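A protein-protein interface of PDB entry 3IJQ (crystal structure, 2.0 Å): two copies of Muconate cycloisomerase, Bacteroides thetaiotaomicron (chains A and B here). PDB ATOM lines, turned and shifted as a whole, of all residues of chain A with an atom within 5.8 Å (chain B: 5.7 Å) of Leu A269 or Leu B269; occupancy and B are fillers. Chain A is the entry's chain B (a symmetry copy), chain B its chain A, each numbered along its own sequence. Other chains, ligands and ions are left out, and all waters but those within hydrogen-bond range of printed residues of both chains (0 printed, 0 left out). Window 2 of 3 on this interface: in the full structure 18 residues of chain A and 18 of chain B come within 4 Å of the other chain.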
ATOM      1  N   LEU A 237     -21.732  23.437  -1.184  1.00  0.00           N
ATOM      2  CA  LEU A 237     -22.889  23.159  -2.039  1.00  0.00           C
ATOM      3  C   LEU A 237     -23.928  24.281  -2.043  1.00  0.00           C
ATOM      4  O   LEU A 237     -24.450  24.663  -3.096  1.00  0.00           O
ATOM      5  CB  LEU A 237     -23.556  21.854  -1.587  1.00  0.00           C
ATOM      6  CG  LEU A 237     -24.711  21.298  -2.433  1.00  0.00           C
ATOM      7  CD1 LEU A 237     -24.225  20.969  -3.847  1.00  0.00           C
ATOM      8  CD2 LEU A 237     -25.271  20.058  -1.757  1.00  0.00           C
ATOM      9  N   GLY A 238     -24.220  24.811  -0.859  1.00  0.00           N
ATOM     10  CA  GLY A 238     -25.203  25.872  -0.745  1.00  0.00           C
ATOM     11  C   GLY A 238     -24.784  27.210  -1.320  1.00  0.00           C
ATOM     12  O   GLY A 238     -25.549  28.166  -1.259  1.00  0.00           O
ATOM     13  N   VAL A 240     -23.444  27.331  -4.526  1.00  0.00           N
ATOM     14  CA  VAL A 240     -23.397  27.127  -5.966  1.00  0.00           C
ATOM     15  C   VAL A 240     -24.477  27.798  -6.799  1.00  0.00           C
ATOM     16  O   VAL A 240     -24.165  28.516  -7.746  1.00  0.00           O
ATOM     17  CB  VAL A 240     -23.402  25.617  -6.314  1.00  0.00           C
ATOM     18  CG1 VAL A 240     -23.412  25.429  -7.827  1.00  0.00           C
ATOM     19  CG2 VAL A 240     -22.190  24.935  -5.705  1.00  0.00           C
ATOM     20  N   ALA A 241     -25.739  27.546  -6.469  1.00  0.00           N
ATOM     21  CA  ALA A 241     -26.854  28.114  -7.227  1.00  0.00           C
ATOM     22  C   ALA A 241     -26.776  29.632  -7.364  1.00  0.00           C
ATOM     23  O   ALA A 241     -27.092  30.184  -8.416  1.00  0.00           O
ATOM     24  CB  ALA A 241     -28.174  27.717  -6.582  1.00  0.00           C
ATOM     25  N   TRP A 264     -18.941  15.727  -4.762  1.00  0.00           N
ATOM     26  CA  TRP A 264     -19.653  14.983  -5.798  1.00  0.00           C
ATOM     27  C   TRP A 264     -21.017  15.620  -6.028  1.00  0.00           C
ATOM     28  O   TRP A 264     -21.482  15.706  -7.162  1.00  0.00           O
ATOM     29  CB  TRP A 264     -19.801  13.510  -5.389  1.00  0.00           C
ATOM     30  CG  TRP A 264     -20.424  12.610  -6.437  1.00  0.00           C
ATOM     31  CD1 TRP A 264     -21.474  11.761  -6.257  1.00  0.00           C
ATOM     32  CD2 TRP A 264     -20.005  12.443  -7.803  1.00  0.00           C
ATOM     33  NE1 TRP A 264     -21.737  11.072  -7.423  1.00  0.00           N
ATOM     34  CE2 TRP A 264     -20.850  11.475  -8.384  1.00  0.00           C
ATOM     35  CE3 TRP A 264     -18.999  13.018  -8.589  1.00  0.00           C
ATOM     36  CZ2 TRP A 264     -20.718  11.065  -9.729  1.00  0.00           C
ATOM     37  CZ3 TRP A 264     -18.867  12.608  -9.925  1.00  0.00           C
ATOM     38  CH2 TRP A 264     -19.726  11.641 -10.477  1.00  0.00           C
ATOM     39  N   LYS A 265     -21.653  16.071  -4.948  1.00  0.00           N
ATOM     40  CA  LYS A 265     -22.958  16.702  -5.067  1.00  0.00           C
ATOM     41  C   LYS A 265     -22.825  18.018  -5.800  1.00  0.00           C
ATOM     42  O   LYS A 265     -23.719  18.400  -6.557  1.00  0.00           O
ATOM     43  CB  LYS A 265     -23.585  16.950  -3.694  1.00  0.00           C
ATOM     44  CG  LYS A 265     -24.105  15.710  -2.999  1.00  0.00           C
ATOM     45  CD  LYS A 265     -24.699  16.103  -1.662  1.00  0.00           C
ATOM     46  CE  LYS A 265     -25.265  14.921  -0.914  1.00  0.00           C
ATOM     47  NZ  LYS A 265     -25.803  15.336   0.423  1.00  0.00           N
ATOM     48  N   MET A 266     -21.709  18.711  -5.582  1.00  0.00           N
ATOM     49  CA  MET A 266     -21.481  19.991  -6.239  1.00  0.00           C
ATOM     50  C   MET A 266     -21.291  19.795  -7.738  1.00  0.00           C
ATOM     51  O   MET A 266     -21.743  20.618  -8.538  1.00  0.00           O
ATOM     52  CB  MET A 266     -20.276  20.705  -5.619  1.00  0.00           C
ATOM     53  CG  MET A 266     -20.506  21.121  -4.169  1.00  0.00           C
ATOM     54  SD  MET A 266     -19.024  21.772  -3.362  1.00  0.00           S
ATOM     55  CE  MET A 266     -18.996  23.430  -3.948  1.00  0.00           C
ATOM     56  N   VAL A 267     -20.627  18.710  -8.120  1.00  0.00           N
ATOM     57  CA  VAL A 267     -20.427  18.415  -9.538  1.00  0.00           C
ATOM     58  C   VAL A 267     -21.798  18.237 -10.187  1.00  0.00           C
ATOM     59  O   VAL A 267     -22.076  18.815 -11.239  1.00  0.00           O
ATOM     60  CB  VAL A 267     -19.645  17.104  -9.763  1.00  0.00           C
ATOM     61  CG1 VAL A 267     -19.606  16.783 -11.254  1.00  0.00           C
ATOM     62  CG2 VAL A 267     -18.230  17.232  -9.227  1.00  0.00           C
ATOM     63  N   THR A 268     -22.646  17.435  -9.542  1.00  0.00           N
ATOM     64  CA  THR A 268     -23.995  17.160 -10.038  1.00  0.00           C
ATOM     65  C   THR A 268     -24.835  18.430 -10.128  1.00  0.00           C
ATOM     66  O   THR A 268     -25.499  18.668 -11.140  1.00  0.00           O
ATOM     67  CB  THR A 268     -24.741  16.155  -9.130  1.00  0.00           C
ATOM     68  OG1 THR A 268     -23.981  14.944  -9.015  1.00  0.00           O
ATOM     69  CG2 THR A 268     -26.103  15.826  -9.720  1.00  0.00           C
ATOM     70  N   LEU A 269     -24.808  19.240  -9.071  1.00  0.00           N
ATOM     71  CA  LEU A 269     -25.566  20.487  -9.036  1.00  0.00           C
ATOM     72  C   LEU A 269     -25.068  21.477 -10.091  1.00  0.00           C
ATOM     73  O   LEU A 269     -25.859  22.047 -10.845  1.00  0.00           O
ATOM     74  CB  LEU A 269     -25.474  21.134  -7.647  1.00  0.00           C
ATOM     75  CG  LEU A 269     -26.103  22.529  -7.483  1.00  0.00           C
ATOM     76  CD1 LEU A 269     -27.587  22.457  -7.756  1.00  0.00           C
ATOM     77  CD2 LEU A 269     -25.859  23.061  -6.076  1.00  0.00           C
ATOM     78  N   ALA A 270     -23.755  21.681 -10.140  1.00  0.00           N
ATOM     79  CA  ALA A 270     -23.173  22.604 -11.101  1.00  0.00           C
ATOM     80  C   ALA A 270     -23.599  22.250 -12.520  1.00  0.00           C
ATOM     81  O   ALA A 270     -24.086  23.102 -13.259  1.00  0.00           O
ATOM     82  CB  ALA A 270     -21.653  22.595 -10.985  1.00  0.00           C
ATOM     83  N   HIS A 271     -23.420  20.986 -12.893  1.00  0.00           N
ATOM     84  CA  HIS A 271     -23.787  20.519 -14.225  1.00  0.00           C
ATOM     85  C   HIS A 271     -25.274  20.651 -14.497  1.00  0.00           C
ATOM     86  O   HIS A 271     -25.678  21.047 -15.590  1.00  0.00           O
ATOM     87  CB  HIS A 271     -23.351  19.064 -14.413  1.00  0.00           C
ATOM     88  CG  HIS A 271     -21.888  18.903 -14.699  1.00  0.00           C
ATOM     89  ND1 HIS A 271     -21.243  17.688 -14.628  1.00  0.00           N
ATOM     90  CD2 HIS A 271     -20.947  19.806 -15.071  1.00  0.00           C
ATOM     91  CE1 HIS A 271     -19.970  17.849 -14.941  1.00  0.00           C
ATOM     92  NE2 HIS A 271     -19.766  19.124 -15.214  1.00  0.00           N
ATOM     93  N   ALA A 272     -26.093  20.320 -13.506  1.00  0.00           N
ATOM     94  CA  ALA A 272     -27.542  20.413 -13.666  1.00  0.00           C
ATOM     95  C   ALA A 272     -27.966  21.843 -14.002  1.00  0.00           C
ATOM     96  O   ALA A 272     -28.963  22.058 -14.691  1.00  0.00           O
ATOM     97  CB  ALA A 272     -28.239  19.941 -12.397  1.00  0.00           C
ATOM     98  N   LEU A 273     -27.201  22.815 -13.512  1.00  0.00           N
ATOM     99  CA  LEU A 273     -27.485  24.226 -13.750  1.00  0.00           C
ATOM    100  C   LEU A 273     -26.708  24.768 -14.954  1.00  0.00           C
ATOM    101  O   LEU A 273     -26.585  25.980 -15.131  1.00  0.00           O
ATOM    102  CB  LEU A 273     -27.135  25.050 -12.504  1.00  0.00           C
ATOM    103  CG  LEU A 273     -27.853  24.697 -11.197  1.00  0.00           C
ATOM    104  CD1 LEU A 273     -27.418  25.661 -10.099  1.00  0.00           C
ATOM    105  CD2 LEU A 273     -29.362  24.765 -11.405  1.00  0.00           C
ATOM    106  N   GLY A 274     -26.177  23.865 -15.772  1.00  0.00           N
ATOM    107  CA  GLY A 274     -25.437  24.274 -16.953  1.00  0.00           C
ATOM    108  C   GLY A 274     -24.074  24.883 -16.700  1.00  0.00           C
ATOM    109  O   GLY A 274     -23.437  25.377 -17.626  1.00  0.00           O
ATOM    110  N   LEU B 237     -34.246  15.218 -14.996  1.00  0.00           N
ATOM    111  CA  LEU B 237     -33.357  16.127 -14.272  1.00  0.00           C
ATOM    112  C   LEU B 237     -33.431  17.565 -14.795  1.00  0.00           C
ATOM    113  O   LEU B 237     -33.632  18.507 -14.031  1.00  0.00           O
ATOM    114  CB  LEU B 237     -31.912  15.617 -14.365  1.00  0.00           C
ATOM    115  CG  LEU B 237     -30.807  16.387 -13.631  1.00  0.00           C
ATOM    116  CD1 LEU B 237     -31.043  16.332 -12.122  1.00  0.00           C
ATOM    117  CD2 LEU B 237     -29.456  15.791 -13.977  1.00  0.00           C
ATOM    118  N   VAL B 240     -36.179  19.939 -13.380  1.00  0.00           N
ATOM    119  CA  VAL B 240     -36.304  20.239 -11.963  1.00  0.00           C
ATOM    120  C   VAL B 240     -36.130  21.705 -11.565  1.00  0.00           C
ATOM    121  O   VAL B 240     -37.010  22.280 -10.926  1.00  0.00           O
ATOM    122  CB  VAL B 240     -35.334  19.363 -11.134  1.00  0.00           C
ATOM    123  CG1 VAL B 240     -35.371  19.773  -9.669  1.00  0.00           C
ATOM    124  CG2 VAL B 240     -35.719  17.894 -11.281  1.00  0.00           C
ATOM    125  N   ALA B 241     -35.001  22.306 -11.933  1.00  0.00           N
ATOM    126  CA  ALA B 241     -34.725  23.700 -11.582  1.00  0.00           C
ATOM    127  C   ALA B 241     -35.852  24.664 -11.957  1.00  0.00           C
ATOM    128  O   ALA B 241     -36.134  25.614 -11.229  1.00  0.00           O
ATOM    129  CB  ALA B 241     -33.417  24.151 -12.230  1.00  0.00           C
ATOM    130  N   TRP B 264     -31.230   9.626  -8.698  1.00  0.00           N
ATOM    131  CA  TRP B 264     -30.349  10.001  -7.600  1.00  0.00           C
ATOM    132  C   TRP B 264     -29.860  11.427  -7.813  1.00  0.00           C
ATOM    133  O   TRP B 264     -29.724  12.192  -6.861  1.00  0.00           O
ATOM    134  CB  TRP B 264     -29.171   9.022  -7.526  1.00  0.00           C
ATOM    135  CG  TRP B 264     -28.279   9.214  -6.330  1.00  0.00           C
ATOM    136  CD1 TRP B 264     -26.930   9.387  -6.341  1.00  0.00           C
ATOM    137  CD2 TRP B 264     -28.675   9.248  -4.948  1.00  0.00           C
ATOM    138  NE1 TRP B 264     -26.454   9.530  -5.055  1.00  0.00           N
ATOM    139  CE2 TRP B 264     -27.505   9.449  -4.182  1.00  0.00           C
ATOM    140  CE3 TRP B 264     -29.903   9.130  -4.286  1.00  0.00           C
ATOM    141  CZ2 TRP B 264     -27.525   9.537  -2.783  1.00  0.00           C
ATOM    142  CZ3 TRP B 264     -29.924   9.218  -2.889  1.00  0.00           C
ATOM    143  CH2 TRP B 264     -28.740   9.419  -2.156  1.00  0.00           C
ATOM    144  N   LYS B 265     -29.607  11.792  -9.069  1.00  0.00           N
ATOM    145  CA  LYS B 265     -29.161  13.150  -9.371  1.00  0.00           C
ATOM    146  C   LYS B 265     -30.321  14.097  -9.098  1.00  0.00           C
ATOM    147  O   LYS B 265     -30.131  15.192  -8.576  1.00  0.00           O
ATOM    148  CB  LYS B 265     -28.737  13.278 -10.835  1.00  0.00           C
ATOM    149  CG  LYS B 265     -27.465  12.537 -11.204  1.00  0.00           C
ATOM    150  CD  LYS B 265     -27.213  12.657 -12.702  1.00  0.00           C
ATOM    151  CE  LYS B 265     -26.081  11.759 -13.190  1.00  0.00           C
ATOM    152  NZ  LYS B 265     -24.728  12.362 -13.005  1.00  0.00           N
ATOM    153  N   MET B 266     -31.529  13.671  -9.452  1.00  0.00           N
ATOM    154  CA  MET B 266     -32.704  14.506  -9.222  1.00  0.00           C
ATOM    155  C   MET B 266     -32.912  14.773  -7.732  1.00  0.00           C
ATOM    156  O   MET B 266     -33.309  15.863  -7.336  1.00  0.00           O
ATOM    157  CB  MET B 266     -33.947  13.845  -9.816  1.00  0.00           C
ATOM    158  CG  MET B 266     -33.910  13.729 -11.329  1.00  0.00           C
ATOM    159  SD  MET B 266     -35.412  12.997 -11.991  1.00  0.00           S
ATOM    160  CE  MET B 266     -36.552  14.323 -11.759  1.00  0.00           C
ATOM    161  N   VAL B 267     -32.641  13.777  -6.901  1.00  0.00           N
ATOM    162  CA  VAL B 267     -32.808  13.960  -5.466  1.00  0.00           C
ATOM    163  C   VAL B 267     -31.797  14.993  -4.977  1.00  0.00           C
ATOM    164  O   VAL B 267     -32.135  15.890  -4.209  1.00  0.00           O
ATOM    165  CB  VAL B 267     -32.595  12.637  -4.708  1.00  0.00           C
ATOM    166  CG1 VAL B 267     -32.629  12.881  -3.211  1.00  0.00           C
ATOM    167  CG2 VAL B 267     -33.677  11.642  -5.104  1.00  0.00           C
ATOM    168  N   THR B 268     -30.557  14.867  -5.438  1.00  0.00           N
ATOM    169  CA  THR B 268     -29.509  15.794  -5.039  1.00  0.00           C
ATOM    170  C   THR B 268     -29.855  17.217  -5.471  1.00  0.00           C
ATOM    171  O   THR B 268     -29.743  18.167  -4.687  1.00  0.00           O
ATOM    172  CB  THR B 268     -28.152  15.400  -5.660  1.00  0.00           C
ATOM    173  OG1 THR B 268     -27.820  14.063  -5.276  1.00  0.00           O
ATOM    174  CG2 THR B 268     -27.052  16.327  -5.174  1.00  0.00           C
ATOM    175  N   LEU B 269     -30.279  17.362  -6.721  1.00  0.00           N
ATOM    176  CA  LEU B 269     -30.625  18.673  -7.245  1.00  0.00           C
ATOM    177  C   LEU B 269     -31.752  19.338  -6.469  1.00  0.00           C
ATOM    178  O   LEU B 269     -31.617  20.481  -6.035  1.00  0.00           O
ATOM    179  CB  LEU B 269     -31.009  18.571  -8.721  1.00  0.00           C
ATOM    180  CG  LEU B 269     -31.463  19.888  -9.352  1.00  0.00           C
ATOM    181  CD1 LEU B 269     -30.369  20.937  -9.191  1.00  0.00           C
ATOM    182  CD2 LEU B 269     -31.788  19.671 -10.816  1.00  0.00           C
ATOM    183  N   ALA B 270     -32.861  18.627  -6.296  1.00  0.00           N
ATOM    184  CA  ALA B 270     -34.008  19.168  -5.572  1.00  0.00           C
ATOM    185  C   ALA B 270     -33.611  19.669  -4.181  1.00  0.00           C
ATOM    186  O   ALA B 270     -33.945  20.792  -3.790  1.00  0.00           O
ATOM    187  CB  ALA B 270     -35.103  18.105  -5.462  1.00  0.00           C
ATOM    188  N   HIS B 271     -32.893  18.842  -3.431  1.00  0.00           N
ATOM    189  CA  HIS B 271     -32.463  19.232  -2.092  1.00  0.00           C
ATOM    190  C   HIS B 271     -31.512  20.418  -2.149  1.00  0.00           C
ATOM    191  O   HIS B 271     -31.589  21.327  -1.325  1.00  0.00           O
ATOM    192  CB  HIS B 271     -31.794  18.048  -1.390  1.00  0.00           C
ATOM    193  CG  HIS B 271     -32.762  17.013  -0.905  1.00  0.00           C
ATOM    194  ND1 HIS B 271     -32.389  15.720  -0.614  1.00  0.00           N
ATOM    195  CD2 HIS B 271     -34.093  17.086  -0.655  1.00  0.00           C
ATOM    196  CE1 HIS B 271     -33.446  15.041  -0.207  1.00  0.00           C
ATOM    197  NE2 HIS B 271     -34.493  15.847  -0.222  1.00  0.00           N
ATOM    198  N   ALA B 272     -30.615  20.408  -3.127  1.00  0.00           N
ATOM    199  CA  ALA B 272     -29.660  21.496  -3.286  1.00  0.00           C
ATOM    200  C   ALA B 272     -30.398  22.801  -3.555  1.00  0.00           C
ATOM    201  O   ALA B 272     -29.961  23.869  -3.124  1.00  0.00           O
ATOM    202  CB  ALA B 272     -28.705  21.191  -4.429  1.00  0.00           C
ATOM    203  N   LEU B 273     -31.521  22.707  -4.263  1.00  0.00           N
ATOM    204  CA  LEU B 273     -32.320  23.883  -4.586  1.00  0.00           C
ATOM    205  C   LEU B 273     -33.363  24.203  -3.517  1.00  0.00           C
ATOM    206  O   LEU B 273     -34.240  25.045  -3.729  1.00  0.00           O
ATOM    207  CB  LEU B 273     -33.018  23.696  -5.937  1.00  0.00           C
ATOM    208  CG  LEU B 273     -32.115  23.650  -7.173  1.00  0.00           C
ATOM    209  CD1 LEU B 273     -32.967  23.593  -8.437  1.00  0.00           C
ATOM    210  CD2 LEU B 273     -31.217  24.887  -7.192  1.00  0.00           C
ATOM    211  N   GLY B 274     -33.278  23.523  -2.374  1.00  0.00           N
ATOM    212  CA  GLY B 274     -34.220  23.763  -1.294  1.00  0.00           C
ATOM    213  C   GLY B 274     -35.594  23.123  -1.435  1.00  0.00           C
ATOM    214  O   GLY B 274     -36.497  23.418  -0.647  1.00  0.00           O
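The backbone carbonyl oxygen (O) of Trp B264 lies within hydrogen-bond range of the side-chain hydroxyl (OG1) of Thr B268 (3.1 Å). The backbone carbonyl oxygen (O) of Trp A264 sits at hydrogen-bond distance from the side-chain hydroxyl (OG1) of Thr A268.
Among the printed residues, pairs that only touch across the chains: Lys A265 with Thr B268 (3.7 Å), Thr A268 with Lys B265 (3.8 Å), Leu A269 with Leu B269 (3.5 Å), Leu A269 with Ala B272 (3.7 Å) and Ala A272 with Leu B269 (3.9 Å).
Of the printed residues of chain B, Lys A265 touches Thr B268. Of the printed residues of chain B, Thr A268 touches Lys B265 (3.8 Å). Leu A269 touches just these residues of chain B: Leu B269 and Ala B272. Of the printed residues of chain B, Ala A272 touches Leu B269. Of the printed residues of chain A, Lys B265 touches Thr A268. Of the printed residues of chain A, Thr B268 touches Lys A265. Of chain A, only Leu A269 and Ala A272 come within 4 Å of Leu B269. The nearest residue of chain B that does not touch Leu A269 is Leu B273 (4.4 Å). The nearest residue of chain A that does not touch Leu B269 is Leu A273 (4.5 Å). The nearest printed residue of chain B that does not touch Thr A268 is Thr B268 (4.6 Å).
Of the 14 printed residues of chain B, 4 touch a printed residue of chain A. Printed residues of chain B that touch a printed residue of chain A: Lys B265, Thr B268, Leu B269 and Ala B272. Of the 15 printed residues of chain A, 4 touch a printed residue of chain B. Hydrophobic or aromatic side chains of chain A that line the printed part of chain B: Leu A269 and Ala A272. Among the printed residues, 5 pairs touch across the chains. Among the printed residues, no Asp or Glu carboxylate lies within 4 Å of a Lys or Arg side-chain nitrogen of the other chain.
Lys A265 touches Thr B268, and with the chains exchanged Thr A268 touches Lys B265. Leu B269 touches its own counterpart, Leu A269. Leu A269 touches Ala B272, and with the chains exchanged Ala A272 touches Leu B269. 14 positions are printed for both chains. Of the 5 pairs that touch across the chains among the printed residues, 5 have their exchanged pair printed and touching as well.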
